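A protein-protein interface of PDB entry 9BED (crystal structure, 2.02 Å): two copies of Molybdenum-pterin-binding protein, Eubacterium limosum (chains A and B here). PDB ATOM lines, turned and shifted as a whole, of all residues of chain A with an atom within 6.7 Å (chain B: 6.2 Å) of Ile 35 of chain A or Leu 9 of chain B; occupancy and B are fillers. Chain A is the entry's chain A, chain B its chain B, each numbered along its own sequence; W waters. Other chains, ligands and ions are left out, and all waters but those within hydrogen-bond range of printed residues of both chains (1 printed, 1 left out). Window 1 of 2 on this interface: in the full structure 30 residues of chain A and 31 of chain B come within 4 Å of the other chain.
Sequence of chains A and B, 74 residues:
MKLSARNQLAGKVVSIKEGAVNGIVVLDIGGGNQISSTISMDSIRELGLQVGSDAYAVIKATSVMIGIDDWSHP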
ATOM      1  N   LEU A   9      29.683  -5.072  13.012  1.00  0.00           N
ATOM      2  CA  LEU A   9      30.481  -6.269  12.783  1.00  0.00           C
ATOM      3  C   LEU A   9      31.850  -5.900  12.234  1.00  0.00           C
ATOM      4  O   LEU A   9      31.960  -5.359  11.130  1.00  0.00           O
ATOM      5  CB  LEU A   9      29.754  -7.214  11.838  1.00  0.00           C
ATOM      6  CG  LEU A   9      28.341  -7.586  12.268  1.00  0.00           C
ATOM      7  CD1 LEU A   9      27.550  -8.202  11.121  1.00  0.00           C
ATOM      8  CD2 LEU A   9      28.434  -8.551  13.436  1.00  0.00           C
ATOM      9  N   VAL A  25      31.192  -1.263  -0.765  1.00  0.00           N
ATOM     10  CA  VAL A  25      32.296  -1.727   0.064  1.00  0.00           C
ATOM     11  C   VAL A  25      31.999  -3.160   0.487  1.00  0.00           C
ATOM     12  O   VAL A  25      30.909  -3.455   0.988  1.00  0.00           O
ATOM     13  CB  VAL A  25      32.480  -0.815   1.294  1.00  0.00           C
ATOM     14  CG1 VAL A  25      33.603  -1.350   2.168  1.00  0.00           C
ATOM     15  CG2 VAL A  25      32.718   0.617   0.856  1.00  0.00           C
ATOM     16  N   VAL A  26      32.944  -4.066   0.262  1.00  0.00           N
ATOM     17  CA  VAL A  26      32.825  -5.450   0.706  1.00  0.00           C
ATOM     18  C   VAL A  26      33.767  -5.642   1.883  1.00  0.00           C
ATOM     19  O   VAL A  26      34.968  -5.364   1.761  1.00  0.00           O
ATOM     20  CB  VAL A  26      33.164  -6.443  -0.424  1.00  0.00           C
ATOM     21  CG1 VAL A  26      33.080  -7.865   0.102  1.00  0.00           C
ATOM     22  CG2 VAL A  26      32.220  -6.291  -1.585  1.00  0.00           C
ATOM     23  N   LEU A  27      33.227  -6.145   2.998  1.00  0.00           N
ATOM     24  CA  LEU A  27      33.945  -6.383   4.241  1.00  0.00           C
ATOM     25  C   LEU A  27      33.962  -7.876   4.536  1.00  0.00           C
ATOM     26  O   LEU A  27      32.914  -8.510   4.568  1.00  0.00           O
ATOM     27  CB  LEU A  27      33.226  -5.617   5.377  1.00  0.00           C
ATOM     28  CG  LEU A  27      33.906  -5.096   6.617  1.00  0.00           C
ATOM     29  CD1 LEU A  27      34.855  -3.981   6.083  1.00  0.00           C
ATOM     30  CD2 LEU A  27      32.946  -4.501   7.613  1.00  0.00           C
ATOM     31  N   ASP A  28      35.137  -8.424   4.781  1.00  0.00           N
ATOM     32  CA  ASP A  28      35.284  -9.782   5.288  1.00  0.00           C
ATOM     33  C   ASP A  28      35.143  -9.706   6.807  1.00  0.00           C
ATOM     34  O   ASP A  28      35.996  -9.111   7.481  1.00  0.00           O
ATOM     35  CB  ASP A  28      36.653 -10.332   4.902  1.00  0.00           C
ATOM     36  CG  ASP A  28      36.871 -11.763   5.357  1.00  0.00           C
ATOM     37  OD1 ASP A  28      36.135 -12.238   6.237  1.00  0.00           O
ATOM     38  OD2 ASP A  28      37.839 -12.399   4.897  1.00  0.00           O
ATOM     39  N   ILE A  29      34.082 -10.304   7.347  1.00  0.00           N
ATOM     40  CA  ILE A  29      33.817 -10.230   8.781  1.00  0.00           C
ATOM     41  C   ILE A  29      34.169 -11.525   9.500  1.00  0.00           C
ATOM     42  O   ILE A  29      33.826 -11.684  10.679  1.00  0.00           O
ATOM     43  CB  ILE A  29      32.356  -9.835   9.058  1.00  0.00           C
ATOM     44  CG1 ILE A  29      31.399 -10.853   8.443  1.00  0.00           C
ATOM     45  CG2 ILE A  29      32.090  -8.406   8.564  1.00  0.00           C
ATOM     46  CD1 ILE A  29      29.983 -10.735   9.018  1.00  0.00           C
ATOM     47  N   GLY A  32      34.022 -16.989   7.152  1.00  0.00           N
ATOM     48  CA  GLY A  32      33.637 -17.136   5.763  1.00  0.00           C
ATOM     49  C   GLY A  32      32.565 -16.182   5.297  1.00  0.00           C
ATOM     50  O   GLY A  32      32.081 -16.324   4.174  1.00  0.00           O
ATOM     51  N   ASN A  33      32.223 -15.171   6.084  1.00  0.00           N
ATOM     52  CA  ASN A  33      31.165 -14.241   5.714  1.00  0.00           C
ATOM     53  C   ASN A  33      31.731 -12.910   5.217  1.00  0.00           C
ATOM     54  O   ASN A  33      32.720 -12.388   5.754  1.00  0.00           O
ATOM     55  CB  ASN A  33      30.249 -13.964   6.908  1.00  0.00           C
ATOM     56  CG  ASN A  33      29.415 -15.183   7.329  1.00  0.00           C
ATOM     57  OD1 ASN A  33      28.879 -15.923   6.511  1.00  0.00           O
ATOM     58  ND2 ASN A  33      29.319 -15.381   8.627  1.00  0.00           N
ATOM     59  N   GLN A  34      31.075 -12.348   4.204  1.00  0.00           N
ATOM     60  CA  GLN A  34      31.365 -11.015   3.699  1.00  0.00           C
ATOM     61  C   GLN A  34      30.070 -10.218   3.746  1.00  0.00           C
ATOM     62  O   GLN A  34      28.971 -10.790   3.704  1.00  0.00           O
ATOM     63  CB  GLN A  34      31.937 -11.104   2.290  1.00  0.00           C
ATOM     64  CG  GLN A  34      33.188 -11.962   2.282  1.00  0.00           C
ATOM     65  CD  GLN A  34      33.933 -11.897   0.972  1.00  0.00           C
ATOM     66  OE1 GLN A  34      33.357 -11.547  -0.060  1.00  0.00           O
ATOM     67  NE2 GLN A  34      35.232 -12.220   1.012  1.00  0.00           N
ATOM     68  N   ILE A  35      30.204  -8.912   3.951  1.00  0.00           N
ATOM     69  CA  ILE A  35      29.072  -7.999   3.959  1.00  0.00           C
ATOM     70  C   ILE A  35      29.334  -6.912   2.931  1.00  0.00           C
ATOM     71  O   ILE A  35      30.406  -6.295   2.934  1.00  0.00           O
ATOM     72  CB  ILE A  35      28.836  -7.381   5.349  1.00  0.00           C
ATOM     73  CG1 ILE A  35      28.549  -8.500   6.347  1.00  0.00           C
ATOM     74  CG2 ILE A  35      27.697  -6.350   5.249  1.00  0.00           C
ATOM     75  CD1 ILE A  35      27.156  -8.782   6.530  1.00  0.00           C
ATOM     76  N   SER A  36      28.350  -6.668   2.073  1.00  0.00           N
ATOM     77  CA  SER A  36      28.393  -5.584   1.108  1.00  0.00           C
ATOM     78  C   SER A  36      27.561  -4.409   1.599  1.00  0.00           C
ATOM     79  O   SER A  36      26.432  -4.587   2.059  1.00  0.00           O
ATOM     80  CB  SER A  36      27.873  -6.014  -0.280  1.00  0.00           C
ATOM     81  OG  SER A  36      28.638  -7.047  -0.863  1.00  0.00           O
ATOM     82  N   SER A  37      28.109  -3.206   1.425  1.00  0.00           N
ATOM     83  CA  SER A  37      27.547  -1.950   1.892  1.00  0.00           C
ATOM     84  C   SER A  37      27.521  -0.952   0.740  1.00  0.00           C
ATOM     85  O   SER A  37      28.576  -0.600   0.194  1.00  0.00           O
ATOM     86  CB  SER A  37      28.388  -1.369   3.033  1.00  0.00           C
ATOM     87  OG  SER A  37      28.091  -0.023   3.303  1.00  0.00           O
ATOM     88  N   ALA A  57      30.762  -3.253   9.659  1.00  0.00           N
ATOM     89  CA  ALA A  57      29.473  -3.243   8.979  1.00  0.00           C
ATOM     90  C   ALA A  57      28.414  -2.919  10.019  1.00  0.00           C
ATOM     91  O   ALA A  57      28.263  -3.656  10.994  1.00  0.00           O
ATOM     92  CB  ALA A  57      29.193  -4.585   8.304  1.00  0.00           C
ATOM     93  N   VAL A  58      27.689  -1.820   9.819  1.00  0.00           N
ATOM     94  CA  VAL A  58      26.744  -1.317  10.809  1.00  0.00           C
ATOM     95  C   VAL A  58      25.341  -1.424  10.224  1.00  0.00           C
ATOM     96  O   VAL A  58      25.047  -0.815   9.194  1.00  0.00           O
ATOM     97  CB  VAL A  58      27.065   0.133  11.214  1.00  0.00           C
ATOM     98  CG1 VAL A  58      26.007   0.675  12.182  1.00  0.00           C
ATOM     99  CG2 VAL A  58      28.489   0.256  11.811  1.00  0.00           C
ATOM    100  N   ILE A  59      24.468  -2.171  10.895  1.00  0.00           N
ATOM    101  CA  ILE A  59      23.134  -2.467  10.386  1.00  0.00           C
ATOM    102  C   ILE A  59      22.121  -2.350  11.520  1.00  0.00           C
ATOM    103  O   ILE A  59      22.223  -3.060  12.535  1.00  0.00           O
ATOM    104  CB  ILE A  59      23.047  -3.874   9.763  1.00  0.00           C
ATOM    105  CG1 ILE A  59      24.221  -4.073   8.816  1.00  0.00           C
ATOM    106  CG2 ILE A  59      21.734  -4.046   9.051  1.00  0.00           C
ATOM    107  CD1 ILE A  59      24.668  -5.490   8.766  1.00  0.00           C
ATOM    108  N   ASN B   7      23.385  -9.447   0.988  1.00  0.00           N
ATOM    109  CA  ASN B   7      23.826 -10.126   2.206  1.00  0.00           C
ATOM    110  C   ASN B   7      22.810 -11.169   2.625  1.00  0.00           C
ATOM    111  O   ASN B   7      21.679 -10.828   2.974  1.00  0.00           O
ATOM    112  CB  ASN B   7      24.035  -9.093   3.303  1.00  0.00           C
ATOM    113  CG  ASN B   7      24.964  -7.990   2.854  1.00  0.00           C
ATOM    114  OD1 ASN B   7      26.150  -8.230   2.599  1.00  0.00           O
ATOM    115  ND2 ASN B   7      24.435  -6.787   2.732  1.00  0.00           N
ATOM    116  N   GLN B   8      23.216 -12.427   2.619  1.00  0.00           N
ATOM    117  CA  GLN B   8      22.339 -13.547   2.983  1.00  0.00           C
ATOM    118  C   GLN B   8      23.198 -14.520   3.790  1.00  0.00           C
ATOM    119  O   GLN B   8      23.819 -15.424   3.232  1.00  0.00           O
ATOM    120  CB  GLN B   8      21.757 -14.180   1.728  1.00  0.00           C
ATOM    121  CG  GLN B   8      20.997 -13.180   0.868  1.00  0.00           C
ATOM    122  CD  GLN B   8      20.453 -13.785  -0.415  1.00  0.00           C
ATOM    123  OE1 GLN B   8      20.223 -14.993  -0.493  1.00  0.00           O
ATOM    124  NE2 GLN B   8      20.257 -12.935  -1.443  1.00  0.00           N
ATOM    125  N   LEU B   9      23.194 -14.361   5.110  1.00  0.00           N
ATOM    126  CA  LEU B   9      24.186 -14.960   5.998  1.00  0.00           C
ATOM    127  C   LEU B   9      23.551 -16.086   6.796  1.00  0.00           C
ATOM    128  O   LEU B   9      22.650 -15.843   7.618  1.00  0.00           O
ATOM    129  CB  LEU B   9      24.752 -13.893   6.939  1.00  0.00           C
ATOM    130  CG  LEU B   9      25.292 -12.696   6.163  1.00  0.00           C
ATOM    131  CD1 LEU B   9      25.519 -11.528   7.036  1.00  0.00           C
ATOM    132  CD2 LEU B   9      26.581 -13.124   5.482  1.00  0.00           C
ATOM    133  N   ALA B  10      24.029 -17.301   6.567  1.00  0.00           N
ATOM    134  CA  ALA B  10      23.453 -18.467   7.227  1.00  0.00           C
ATOM    135  C   ALA B  10      23.788 -18.452   8.707  1.00  0.00           C
ATOM    136  O   ALA B  10      24.882 -18.062   9.120  1.00  0.00           O
ATOM    137  CB  ALA B  10      23.957 -19.767   6.571  1.00  0.00           C
ATOM    138  N   GLY B  11      22.838 -18.889   9.517  1.00  0.00           N
ATOM    139  CA  GLY B  11      23.119 -18.970  10.933  1.00  0.00           C
ATOM    140  C   GLY B  11      22.031 -19.739  11.640  1.00  0.00           C
ATOM    141  O   GLY B  11      21.078 -20.219  11.026  1.00  0.00           O
ATOM    142  N   LEU B  27      20.664 -14.355  15.476  1.00  0.00           N
ATOM    143  CA  LEU B  27      21.261 -15.431  14.710  1.00  0.00           C
ATOM    144  C   LEU B  27      22.761 -15.484  14.947  1.00  0.00           C
ATOM    145  O   LEU B  27      23.439 -14.464  14.838  1.00  0.00           O
ATOM    146  CB  LEU B  27      20.992 -15.209  13.221  1.00  0.00           C
ATOM    147  CG  LEU B  27      19.734 -15.702  12.546  1.00  0.00           C
ATOM    148  CD1 LEU B  27      20.116 -15.702  11.016  1.00  0.00           C
ATOM    149  CD2 LEU B  27      19.309 -17.045  13.037  1.00  0.00           C
ATOM    150  N   ILE B  29      25.995 -16.398  13.266  1.00  0.00           N
ATOM    151  CA  ILE B  29      26.391 -16.614  11.877  1.00  0.00           C
ATOM    152  C   ILE B  29      27.813 -17.154  11.754  1.00  0.00           C
ATOM    153  O   ILE B  29      28.335 -17.273  10.635  1.00  0.00           O
ATOM    154  CB  ILE B  29      26.227 -15.330  11.031  1.00  0.00           C
ATOM    155  CG1 ILE B  29      27.088 -14.200  11.575  1.00  0.00           C
ATOM    156  CG2 ILE B  29      24.739 -14.900  10.946  1.00  0.00           C
ATOM    157  CD1 ILE B  29      27.289 -13.032  10.576  1.00  0.00           C
ATOM    158  N   ILE B  35      23.799 -11.622  14.587  1.00  0.00           N
ATOM    159  CA  ILE B  35      23.016 -10.584  13.942  1.00  0.00           C
ATOM    160  C   ILE B  35      21.635 -10.574  14.566  1.00  0.00           C
ATOM    161  O   ILE B  35      21.007 -11.630  14.725  1.00  0.00           O
ATOM    162  CB  ILE B  35      22.940 -10.767  12.412  1.00  0.00           C
ATOM    163  CG1 ILE B  35      24.330 -10.595  11.796  1.00  0.00           C
ATOM    164  CG2 ILE B  35      21.963  -9.763  11.810  1.00  0.00           C
ATOM    165  CD1 ILE B  35      24.371 -10.674  10.281  1.00  0.00           C
ATOM    166  N   ALA B  55      18.577 -20.644   9.779  1.00  0.00           N
ATOM    167  CA  ALA B  55      17.949 -19.534   9.084  1.00  0.00           C
ATOM    168  C   ALA B  55      19.018 -18.709   8.386  1.00  0.00           C
ATOM    169  O   ALA B  55      20.200 -19.076   8.359  1.00  0.00           O
ATOM    170  CB  ALA B  55      17.124 -18.683  10.050  1.00  0.00           C
ATOM    171  N   TYR B  56      18.595 -17.568   7.848  1.00  0.00           N
ATOM    172  CA  TYR B  56      19.484 -16.633   7.171  1.00  0.00           C
ATOM    173  C   TYR B  56      19.156 -15.218   7.616  1.00  0.00           C
ATOM    174  O   TYR B  56      17.982 -14.874   7.736  1.00  0.00           O
ATOM    175  CB  TYR B  56      19.351 -16.682   5.642  1.00  0.00           C
ATOM    176  CG  TYR B  56      19.652 -18.014   5.017  1.00  0.00           C
ATOM    177  CD1 TYR B  56      18.685 -18.995   4.940  1.00  0.00           C
ATOM    178  CD2 TYR B  56      20.904 -18.277   4.497  1.00  0.00           C
ATOM    179  CE1 TYR B  56      18.954 -20.227   4.383  1.00  0.00           C
ATOM    180  CE2 TYR B  56      21.198 -19.512   3.929  1.00  0.00           C
ATOM    181  CZ  TYR B  56      20.214 -20.475   3.860  1.00  0.00           C
ATOM    182  OH  TYR B  56      20.502 -21.694   3.292  1.00  0.00           O
ATOM    183  N   ALA B  57      20.198 -14.400   7.821  1.00  0.00           N
ATOM    184  CA  ALA B  57      20.064 -12.962   8.012  1.00  0.00           C
ATOM    185  C   ALA B  57      20.218 -12.300   6.649  1.00  0.00           C
ATOM    186  O   ALA B  57      21.256 -12.456   6.002  1.00  0.00           O
ATOM    187  CB  ALA B  57      21.111 -12.447   8.991  1.00  0.00           C
ATOM    188  N   VAL B  58      19.195 -11.572   6.217  1.00  0.00           N
ATOM    189  CA  VAL B  58      19.103 -11.044   4.853  1.00  0.00           C
ATOM    190  C   VAL B  58      19.083  -9.530   4.935  1.00  0.00           C
ATOM    191  O   VAL B  58      18.222  -8.958   5.621  1.00  0.00           O
ATOM    192  CB  VAL B  58      17.839 -11.562   4.147  1.00  0.00           C
ATOM    193  CG1 VAL B  58      17.697 -10.975   2.764  1.00  0.00           C
ATOM    194  CG2 VAL B  58      17.864 -13.100   4.088  1.00  0.00           C
ATOM    195  N   ILE B  59      20.046  -8.876   4.290  1.00  0.00           N
ATOM    196  CA  ILE B  59      20.195  -7.426   4.409  1.00  0.00           C
ATOM    197  C   ILE B  59      20.516  -6.845   3.043  1.00  0.00           C
ATOM    198  O   ILE B  59      21.496  -7.247   2.392  1.00  0.00           O
ATOM    199  CB  ILE B  59      21.296  -7.031   5.403  1.00  0.00           C
ATOM    200  CG1 ILE B  59      21.121  -7.879   6.677  1.00  0.00           C
ATOM    201  CG2 ILE B  59      21.235  -5.509   5.700  1.00  0.00           C
ATOM    202  CD1 ILE B  59      22.395  -8.241   7.346  1.00  0.00           C
ATOM    203  N   VAL B  64      23.290  -1.094   4.739  1.00  0.00           N
ATOM    204  CA  VAL B  64      24.511  -1.343   5.495  1.00  0.00           C
ATOM    205  C   VAL B  64      25.364  -0.095   5.464  1.00  0.00           C
ATOM    206  O   VAL B  64      25.679   0.412   4.385  1.00  0.00           O
ATOM    207  CB  VAL B  64      25.298  -2.537   4.935  1.00  0.00           C
ATOM    208  CG1 VAL B  64      26.526  -2.774   5.805  1.00  0.00           C
ATOM    209  CG2 VAL B  64      24.436  -3.761   4.914  1.00  0.00           C
ATOM    210  N   ILE B  66      29.073   1.772   6.908  1.00  0.00           N
ATOM    211  CA  ILE B  66      30.433   1.432   7.309  1.00  0.00           C
ATOM    212  C   ILE B  66      30.881   2.352   8.435  1.00  0.00           C
ATOM    213  O   ILE B  66      30.653   3.569   8.392  1.00  0.00           O
ATOM    214  CB  ILE B  66      31.454   1.475   6.154  1.00  0.00           C
ATOM    215  CG1 ILE B  66      31.144   0.445   5.073  1.00  0.00           C
ATOM    216  CG2 ILE B  66      32.877   1.213   6.725  1.00  0.00           C
ATOM    217  CD1 ILE B  66      31.253  -1.012   5.577  1.00  0.00           C
HETATM  218  O   HOH W   1      27.273 -11.197   1.924  1.00  0.00           O
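Among the printed residues, merely in contact across the chains: Ile 29 of chain A with Ile 29 of chain B (3.9 Å), Asn 33 of chain A with Leu 9 of chain B (3.8 Å), Gln 34 of chain A with Asn 7 of chain B (3.97 Å), Gln 34 of chain A with Leu 9 of chain B (3.8 Å), Ile 35 of chain A with Asn 7 of chain B (3.2 Å), Ile 35 of chain A with Leu 9 of chain B (3.2 Å), Ile 35 of chain A with Val 64 of chain B (3.8 Å), Ser 36 of chain A with Val 64 of chain B (3.6 Å), Ser 37 of chain A with Ile 66 of chain B (3.6 Å), Val 58 of chain A with Val 64 of chain B (3.8 Å), Ile 59 of chain A with Ile 59 of chain B (3.7 Å) and Ile 59 of chain A with Val 64 of chain B (3.9 Å).
Ile 29 of chain A touches its own counterpart, Ile 29 of chain B.
Ile 35 of chain A touches Leu 9 of chain B, but with the chains exchanged Leu 9 of chain A does not touch Ile 35 of chain B (4.1 Å).
Ile 59 of chain B touches its own counterpart, Ile 59 of chain A.
7 positions are printed for both chains.
Of the 15 pairs that touch across the chains among the printed residues, 2 have their exchanged pair printed and touching as well.
Water W1 lies within hydrogen-bond range of the backbone carbonyl oxygen (O) of Gln 34 of chain A (2.5 Å) and the side-chain amide oxygen (OD1) of Asn 7 of chain B (3.2 Å).
The backbone carbonyl oxygen of Ile 29 of chain B lies within hydrogen-bond range of the side-chain amide nitrogen of Asn 33 of chain A (2.9 Å).
The backbone NH of Ser 36 of chain A lies within hydrogen-bond range of the side-chain amide oxygen of Asn 7 of chain B (2.7 Å).
The backbone carbonyl oxygen of Val 64 of chain B sits at hydrogen-bond distance from the side-chain hydroxyl of Ser 37 of chain A (2.7 Å).
Printed residues of chain A that touch a printed residue of chain B: Ile 29, Asn 33, Gln 34, Ile 35, Ser 36, Ser 37, Val 58 and Ile 59.
Hydrophobic or aromatic side chains of chain A within 4 Å of the printed part of chain B: Ile 29, Ile 35 and Ile 59.
Of the 15 printed residues of chain B, 6 touch a printed residue of chain A.
Along chain B the printed residues that touch a printed residue of chain A span positions 7 to 66.
Printed residues of chain B within 4 Å of Ile 29 of chain A: Ile 29 (3.9 Å).
Of chain B, only Asn 7 (3.2 Å), Leu 9 (3.2 Å) and Val 64 (3.8 Å) come within 4 Å of Ile 35 of chain A.
Printed residues of chain B within 4 Å of Val 58 of chain A: Val 64.
The nearest residue of chain B that does not touch Ile 35 of chain A is Ile 59 of chain B (4.9 Å).
The nearest residue of chain A that does not touch Leu 9 of chain B is Ile 29 of chain A (4.9 Å).
The backbone carbonyl oxygen (O) of Val 25 of chain A is in hydrogen-bond range of the backbone NH (N) of Ser 37 of chain A, 2.8 Å away.
N of Ala 57 of chain B sits at hydrogen-bond distance from O of Leu 9 of chain B.
The backbone carbonyl oxygen of Leu 27 of chain A lies within hydrogen-bond range of the backbone NH of Ile 35 of chain A.
N of Ile 59 of chain B is in hydrogen-bond range of O of Asn 7 of chain B, 2.9 Å away.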
